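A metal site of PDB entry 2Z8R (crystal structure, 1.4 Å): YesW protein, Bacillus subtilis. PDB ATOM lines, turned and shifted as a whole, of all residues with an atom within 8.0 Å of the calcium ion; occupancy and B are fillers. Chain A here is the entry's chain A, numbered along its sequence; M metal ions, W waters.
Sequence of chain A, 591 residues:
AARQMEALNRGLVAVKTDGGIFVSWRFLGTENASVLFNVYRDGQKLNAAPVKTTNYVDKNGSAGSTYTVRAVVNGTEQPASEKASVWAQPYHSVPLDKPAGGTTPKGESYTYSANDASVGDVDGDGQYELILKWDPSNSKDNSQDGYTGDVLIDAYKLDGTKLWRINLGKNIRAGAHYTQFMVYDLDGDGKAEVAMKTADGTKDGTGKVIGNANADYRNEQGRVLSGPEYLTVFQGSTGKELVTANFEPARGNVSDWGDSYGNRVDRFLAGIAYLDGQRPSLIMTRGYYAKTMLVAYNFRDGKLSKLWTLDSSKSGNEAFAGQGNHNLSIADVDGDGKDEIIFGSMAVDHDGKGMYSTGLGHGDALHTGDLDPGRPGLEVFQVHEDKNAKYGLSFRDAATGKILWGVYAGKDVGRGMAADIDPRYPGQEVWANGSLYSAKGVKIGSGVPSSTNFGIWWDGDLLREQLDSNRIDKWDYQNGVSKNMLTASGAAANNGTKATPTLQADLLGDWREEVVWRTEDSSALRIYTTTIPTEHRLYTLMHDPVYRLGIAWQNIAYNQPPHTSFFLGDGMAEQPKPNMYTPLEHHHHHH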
ATOM      1  N   LEU A 371      31.477   4.142  11.525  1.00  0.00           N
ATOM      2  CA  LEU A 371      30.177   4.768  11.679  1.00  0.00           C
ATOM      3  C   LEU A 371      29.083   3.883  11.098  1.00  0.00           C
ATOM      4  O   LEU A 371      27.981   3.800  11.651  1.00  0.00           O
ATOM      5  CB  LEU A 371      30.175   6.159  11.026  1.00  0.00           C
ATOM      6  CG  LEU A 371      31.349   7.081  11.362  1.00  0.00           C
ATOM      7  CD1 LEU A 371      31.137   8.446  10.702  1.00  0.00           C
ATOM      8  CD2 LEU A 371      31.536   7.228  12.886  1.00  0.00           C
ATOM      9  N   PRO A 373      28.721   0.084  10.402  1.00  0.00           N
ATOM     10  CA  PRO A 373      29.317  -1.234  10.581  1.00  0.00           C
ATOM     11  C   PRO A 373      28.860  -2.243   9.519  1.00  0.00           C
ATOM     12  O   PRO A 373      29.427  -3.317   9.441  1.00  0.00           O
ATOM     13  CB  PRO A 373      28.851  -1.657  11.971  1.00  0.00           C
ATOM     14  CG  PRO A 373      27.557  -0.949  12.171  1.00  0.00           C
ATOM     15  CD  PRO A 373      27.714   0.380  11.450  1.00  0.00           C
ATOM     16  N   ALA A 419      27.401   9.450  16.815  1.00  0.00           N
ATOM     17  CA  ALA A 419      27.257   8.600  17.989  1.00  0.00           C
ATOM     18  C   ALA A 419      26.088   7.654  17.776  1.00  0.00           C
ATOM     19  O   ALA A 419      25.072   8.034  17.196  1.00  0.00           O
ATOM     20  CB  ALA A 419      27.024   9.448  19.260  1.00  0.00           C
ATOM     21  N   ASP A 420      26.237   6.414  18.251  1.00  0.00           N
ATOM     22  CA  ASP A 420      25.114   5.485  18.265  1.00  0.00           C
ATOM     23  C   ASP A 420      24.174   5.868  19.396  1.00  0.00           C
ATOM     24  O   ASP A 420      24.438   5.577  20.556  1.00  0.00           O
ATOM     25  CB  ASP A 420      25.590   4.043  18.427  1.00  0.00           C
ATOM     26  CG  ASP A 420      24.462   3.039  18.281  1.00  0.00           C
ATOM     27  OD1 ASP A 420      23.350   3.471  17.924  1.00  0.00           O
ATOM     28  OD2 ASP A 420      24.695   1.827  18.466  1.00  0.00           O
ATOM     29  N   ILE A 421      23.087   6.558  19.046  1.00  0.00           N
ATOM     30  CA  ILE A 421      22.110   7.023  20.032  1.00  0.00           C
ATOM     31  C   ILE A 421      20.725   6.385  19.833  1.00  0.00           C
ATOM     32  O   ILE A 421      19.842   6.519  20.702  1.00  0.00           O
ATOM     33  CB  ILE A 421      21.952   8.575  20.020  1.00  0.00           C
ATOM     34  CG1 ILE A 421      21.351   9.066  18.691  1.00  0.00           C
ATOM     35  CG2 ILE A 421      23.284   9.248  20.288  1.00  0.00           C
ATOM     36  CD1 ILE A 421      21.071  10.561  18.683  1.00  0.00           C
ATOM     37  N   ASP A 422      20.544   5.691  18.716  1.00  0.00           N
ATOM     38  CA  ASP A 422      19.262   5.110  18.351  1.00  0.00           C
ATOM     39  C   ASP A 422      19.491   3.669  17.931  1.00  0.00           C
ATOM     40  O   ASP A 422      20.090   3.427  16.888  1.00  0.00           O
ATOM     41  CB  ASP A 422      18.626   5.918  17.211  1.00  0.00           C
ATOM     42  CG  ASP A 422      17.176   5.552  16.974  1.00  0.00           C
ATOM     43  OD1 ASP A 422      16.808   4.383  17.226  1.00  0.00           O
ATOM     44  OD2 ASP A 422      16.446   6.445  16.486  1.00  0.00           O
ATOM     45  N   PRO A 423      19.032   2.692  18.735  1.00  0.00           N
ATOM     46  CA  PRO A 423      19.314   1.299  18.377  1.00  0.00           C
ATOM     47  C   PRO A 423      18.414   0.756  17.257  1.00  0.00           C
ATOM     48  O   PRO A 423      18.597  -0.393  16.827  1.00  0.00           O
ATOM     49  CB  PRO A 423      19.048   0.544  19.685  1.00  0.00           C
ATOM     50  CG  PRO A 423      17.961   1.342  20.342  1.00  0.00           C
ATOM     51  CD  PRO A 423      18.237   2.797  19.978  1.00  0.00           C
ATOM     52  N   ARG A 424      17.431   1.547  16.835  1.00  0.00           N
ATOM     53  CA  ARG A 424      16.556   1.149  15.730  1.00  0.00           C
ATOM     54  C   ARG A 424      17.250   1.255  14.374  1.00  0.00           C
ATOM     55  O   ARG A 424      16.785   0.688  13.368  1.00  0.00           O
ATOM     56  CB  ARG A 424      15.234   1.941  15.757  1.00  0.00           C
ATOM     57  CG  ARG A 424      14.492   1.850  17.085  1.00  0.00           C
ATOM     58  CD  ARG A 424      13.359   2.873  17.150  1.00  0.00           C
ATOM     59  NE  ARG A 424      13.854   4.222  16.904  1.00  0.00           N
ATOM     60  CZ  ARG A 424      13.088   5.273  16.665  1.00  0.00           C
ATOM     61  NH1 ARG A 424      11.761   5.158  16.671  1.00  0.00           N
ATOM     62  NH2 ARG A 424      13.649   6.451  16.423  1.00  0.00           N
ATOM     63  N   TYR A 425      18.373   1.971  14.327  1.00  0.00           N
ATOM     64  CA  TYR A 425      19.124   2.117  13.085  1.00  0.00           C
ATOM     65  C   TYR A 425      20.521   1.603  13.353  1.00  0.00           C
ATOM     66  O   TYR A 425      21.221   2.131  14.201  1.00  0.00           O
ATOM     67  CB  TYR A 425      19.182   3.578  12.637  1.00  0.00           C
ATOM     68  CG  TYR A 425      17.826   4.168  12.296  1.00  0.00           C
ATOM     69  CD1 TYR A 425      17.376   4.195  10.970  1.00  0.00           C
ATOM     70  CD2 TYR A 425      17.007   4.696  13.285  1.00  0.00           C
ATOM     71  CE1 TYR A 425      16.150   4.725  10.644  1.00  0.00           C
ATOM     72  CE2 TYR A 425      15.771   5.238  12.968  1.00  0.00           C
ATOM     73  CZ  TYR A 425      15.361   5.262  11.653  1.00  0.00           C
ATOM     74  OH  TYR A 425      14.128   5.782  11.310  1.00  0.00           O
ATOM     75  N   PRO A 426      20.920   0.514  12.664  1.00  0.00           N
ATOM     76  CA  PRO A 426      22.252  -0.029  12.924  1.00  0.00           C
ATOM     77  C   PRO A 426      23.351   1.022  12.711  1.00  0.00           C
ATOM     78  O   PRO A 426      23.253   1.867  11.808  1.00  0.00           O
ATOM     79  CB  PRO A 426      22.376  -1.177  11.906  1.00  0.00           C
ATOM     80  CG  PRO A 426      20.940  -1.545  11.603  1.00  0.00           C
ATOM     81  CD  PRO A 426      20.179  -0.254  11.657  1.00  0.00           C
ATOM     82  N   GLY A 427      24.346   1.010  13.579  1.00  0.00           N
ATOM     83  CA  GLY A 427      25.496   1.905  13.441  1.00  0.00           C
ATOM     84  C   GLY A 427      25.352   3.227  14.168  1.00  0.00           C
ATOM     85  O   GLY A 427      24.411   3.435  14.940  1.00  0.00           O
ATOM     86  N   GLN A 428      26.311   4.119  13.930  1.00  0.00           N
ATOM     87  CA  GLN A 428      26.277   5.440  14.533  1.00  0.00           C
ATOM     88  C   GLN A 428      25.392   6.385  13.754  1.00  0.00           C
ATOM     89  O   GLN A 428      25.513   6.498  12.514  1.00  0.00           O
ATOM     90  CB  GLN A 428      27.696   6.013  14.636  1.00  0.00           C
ATOM     91  CG  GLN A 428      28.651   5.120  15.420  1.00  0.00           C
ATOM     92  CD  GLN A 428      29.923   5.825  15.812  1.00  0.00           C
ATOM     93  OE1 GLN A 428      29.895   6.959  16.282  1.00  0.00           O
ATOM     94  NE2 GLN A 428      31.053   5.158  15.610  1.00  0.00           N
ATOM     95  N   GLU A 429      24.520   7.073  14.473  1.00  0.00           N
ATOM     96  CA  GLU A 429      23.768   8.186  13.924  1.00  0.00           C
ATOM     97  C   GLU A 429      24.685   9.399  13.814  1.00  0.00           C
ATOM     98  O   GLU A 429      25.720   9.480  14.467  1.00  0.00           O
ATOM     99  CB  GLU A 429      22.575   8.489  14.839  1.00  0.00           C
ATOM    100  CG  GLU A 429      21.429   7.482  14.726  1.00  0.00           C
ATOM    101  CD  GLU A 429      21.783   6.071  15.216  1.00  0.00           C
ATOM    102  OE1 GLU A 429      22.203   5.911  16.402  1.00  0.00           O
ATOM    103  OE2 GLU A 429      21.632   5.104  14.421  1.00  0.00           O
ATOM    104  N   VAL A 430      24.303  10.345  12.964  1.00  0.00           N
ATOM    105  CA  VAL A 430      25.029  11.594  12.841  1.00  0.00           C
ATOM    106  C   VAL A 430      24.018  12.735  12.830  1.00  0.00           C
ATOM    107  O   VAL A 430      22.876  12.547  12.388  1.00  0.00           O
ATOM    108  CB  VAL A 430      25.927  11.643  11.567  1.00  0.00           C
ATOM    109  CG1 VAL A 430      26.985  10.528  11.570  1.00  0.00           C
ATOM    110  CG2 VAL A 430      25.100  11.564  10.304  1.00  0.00           C
ATOM    111  N   TYR A 437      20.380  11.868  11.432  1.00  0.00           N
ATOM    112  CA  TYR A 437      20.377  10.886  10.349  1.00  0.00           C
ATOM    113  C   TYR A 437      20.930   9.555  10.794  1.00  0.00           C
ATOM    114  O   TYR A 437      21.797   9.489  11.679  1.00  0.00           O
ATOM    115  CB  TYR A 437      21.275  11.359   9.189  1.00  0.00           C
ATOM    116  CG  TYR A 437      20.917  12.693   8.612  1.00  0.00           C
ATOM    117  CD1 TYR A 437      20.074  12.795   7.503  1.00  0.00           C
ATOM    118  CD2 TYR A 437      21.430  13.876   9.163  1.00  0.00           C
ATOM    119  CE1 TYR A 437      19.743  14.033   6.948  1.00  0.00           C
ATOM    120  CE2 TYR A 437      21.108  15.115   8.628  1.00  0.00           C
ATOM    121  CZ  TYR A 437      20.260  15.193   7.523  1.00  0.00           C
ATOM    122  OH  TYR A 437      19.935  16.442   6.984  1.00  0.00           O
ATOM    123  N   SER A 438      20.494   8.483  10.138  1.00  0.00           N
ATOM    124  CA  SER A 438      21.151   7.202  10.297  1.00  0.00           C
ATOM    125  C   SER A 438      22.486   7.242   9.554  1.00  0.00           C
ATOM    126  O   SER A 438      22.754   8.169   8.776  1.00  0.00           O
ATOM    127  CB  SER A 438      20.298   6.081   9.710  1.00  0.00           C
ATOM    128  OG  SER A 438      20.332   6.132   8.281  1.00  0.00           O
ATOM    129  N   ALA A 439      23.305   6.215   9.773  1.00  0.00           N
ATOM    130  CA  ALA A 439      24.569   6.101   9.061  1.00  0.00           C
ATOM    131  C   ALA A 439      24.380   6.008   7.530  1.00  0.00           C
ATOM    132  O   ALA A 439      25.333   6.206   6.769  1.00  0.00           O
ATOM    133  CB  ALA A 439      25.315   4.906   9.588  1.00  0.00           C
ATOM    134  N   ILE A 444      16.014  10.929  10.701  1.00  0.00           N
ATOM    135  CA  ILE A 444      15.274  10.294  11.779  1.00  0.00           C
ATOM    136  C   ILE A 444      14.445  11.328  12.532  1.00  0.00           C
ATOM    137  O   ILE A 444      14.994  12.271  13.115  1.00  0.00           O
ATOM    138  CB  ILE A 444      16.226   9.587  12.770  1.00  0.00           C
ATOM    139  CG1 ILE A 444      17.076   8.532  12.058  1.00  0.00           C
ATOM    140  CG2 ILE A 444      15.431   9.008  13.968  1.00  0.00           C
ATOM    141  CD1 ILE A 444      18.253   8.011  12.907  1.00  0.00           C
ATOM    142  N   LEU A 463      24.976   2.180  23.798  1.00  0.00           N
ATOM    143  CA  LEU A 463      24.755   3.445  23.104  1.00  0.00           C
ATOM    144  C   LEU A 463      25.695   4.504  23.685  1.00  0.00           C
ATOM    145  O   LEU A 463      26.226   4.327  24.792  1.00  0.00           O
ATOM    146  CB  LEU A 463      23.291   3.885  23.220  1.00  0.00           C
ATOM    147  CG  LEU A 463      22.268   2.879  22.697  1.00  0.00           C
ATOM    148  CD1 LEU A 463      20.853   3.355  23.054  1.00  0.00           C
ATOM    149  CD2 LEU A 463      22.377   2.736  21.187  1.00  0.00           C
ATOM    150  N   PHE A 567      33.319  -0.739  15.644  1.00  0.00           N
ATOM    151  CA  PHE A 567      31.993  -0.280  16.016  1.00  0.00           C
ATOM    152  C   PHE A 567      31.682  -0.718  17.444  1.00  0.00           C
ATOM    153  O   PHE A 567      31.508  -1.905  17.748  1.00  0.00           O
ATOM    154  CB  PHE A 567      30.918  -0.792  15.062  1.00  0.00           C
ATOM    155  CG  PHE A 567      29.508  -0.453  15.522  1.00  0.00           C
ATOM    156  CD1 PHE A 567      29.068   0.860  15.533  1.00  0.00           C
ATOM    157  CD2 PHE A 567      28.648  -1.450  15.958  1.00  0.00           C
ATOM    158  CE1 PHE A 567      27.776   1.192  15.980  1.00  0.00           C
ATOM    159  CE2 PHE A 567      27.363  -1.136  16.412  1.00  0.00           C
ATOM    160  CZ  PHE A 567      26.916   0.182  16.411  1.00  0.00           C
ATOM    161  N   GLY A 569      28.792  -0.206  19.959  1.00  0.00           N
ATOM    162  CA  GLY A 569      27.414   0.260  20.005  1.00  0.00           C
ATOM    163  C   GLY A 569      26.452  -0.901  20.039  1.00  0.00           C
ATOM    164  O   GLY A 569      26.861  -2.059  20.166  1.00  0.00           O
ATOM    165  N   ASP A 570      25.162  -0.590  19.926  1.00  0.00           N
ATOM    166  CA  ASP A 570      24.143  -1.625  20.003  1.00  0.00           C
ATOM    167  C   ASP A 570      24.280  -2.558  18.805  1.00  0.00           C
ATOM    168  O   ASP A 570      24.424  -2.108  17.672  1.00  0.00           O
ATOM    169  CB  ASP A 570      22.774  -0.971  20.019  1.00  0.00           C
ATOM    170  CG  ASP A 570      21.662  -1.988  20.216  1.00  0.00           C
ATOM    171  OD1 ASP A 570      21.447  -2.405  21.379  1.00  0.00           O
ATOM    172  OD2 ASP A 570      21.015  -2.345  19.211  1.00  0.00           O
HETATM  173 CA    CA M   1      22.226   3.339  15.899  1.00  0.00          CA
HETATM  174  O   HOH W   1      22.742   1.049  16.572  1.00  0.00           O
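O of Glu 429 sits at hydrogen-bond distance from N of Ala 419, 2.9 Å away. OD2 of Asp 422 lies within salt-bridge range of NH2 of Arg 424, 2.8 Å away. N of Asp 570 lies within hydrogen-bond range of OD2 of Asp 420 (2.9 Å). OE1 of Glu 429 lies close to N of Ile 421 (2.9 Å).
O of Tyr 425 is bound to the calcium ion, at 2.3 Å. The calcium ion is bound by OD1 of Asp 420 (2.3 Å). O of Asp 422 binds the calcium ion (2.4 Å). The calcium ion is bound by OE2 of Glu 429 (2.4 Å). The calcium ion is bound by the backbone carbonyl oxygen (O) of Gly 427 (2.4 Å). Water W1 is bound to the calcium ion, at 2.4 Å. OE1 of Glu 429 is bound to the calcium ion, 2.6 Å away. The calcium ion has seven donor atoms within binding distance.
Within 4 Å of the calcium ion: Asp 420, Asp 422, Tyr 425, Gly 427 and Glu 429. The nearest printed residue that does not touch the calcium ion is Pro 426 (4.1 Å).
Water W1 bridges the side-chain carboxylate of Asp 420 (2.8 Å) and the backbone NH of Gly 427 (3.4 Å).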
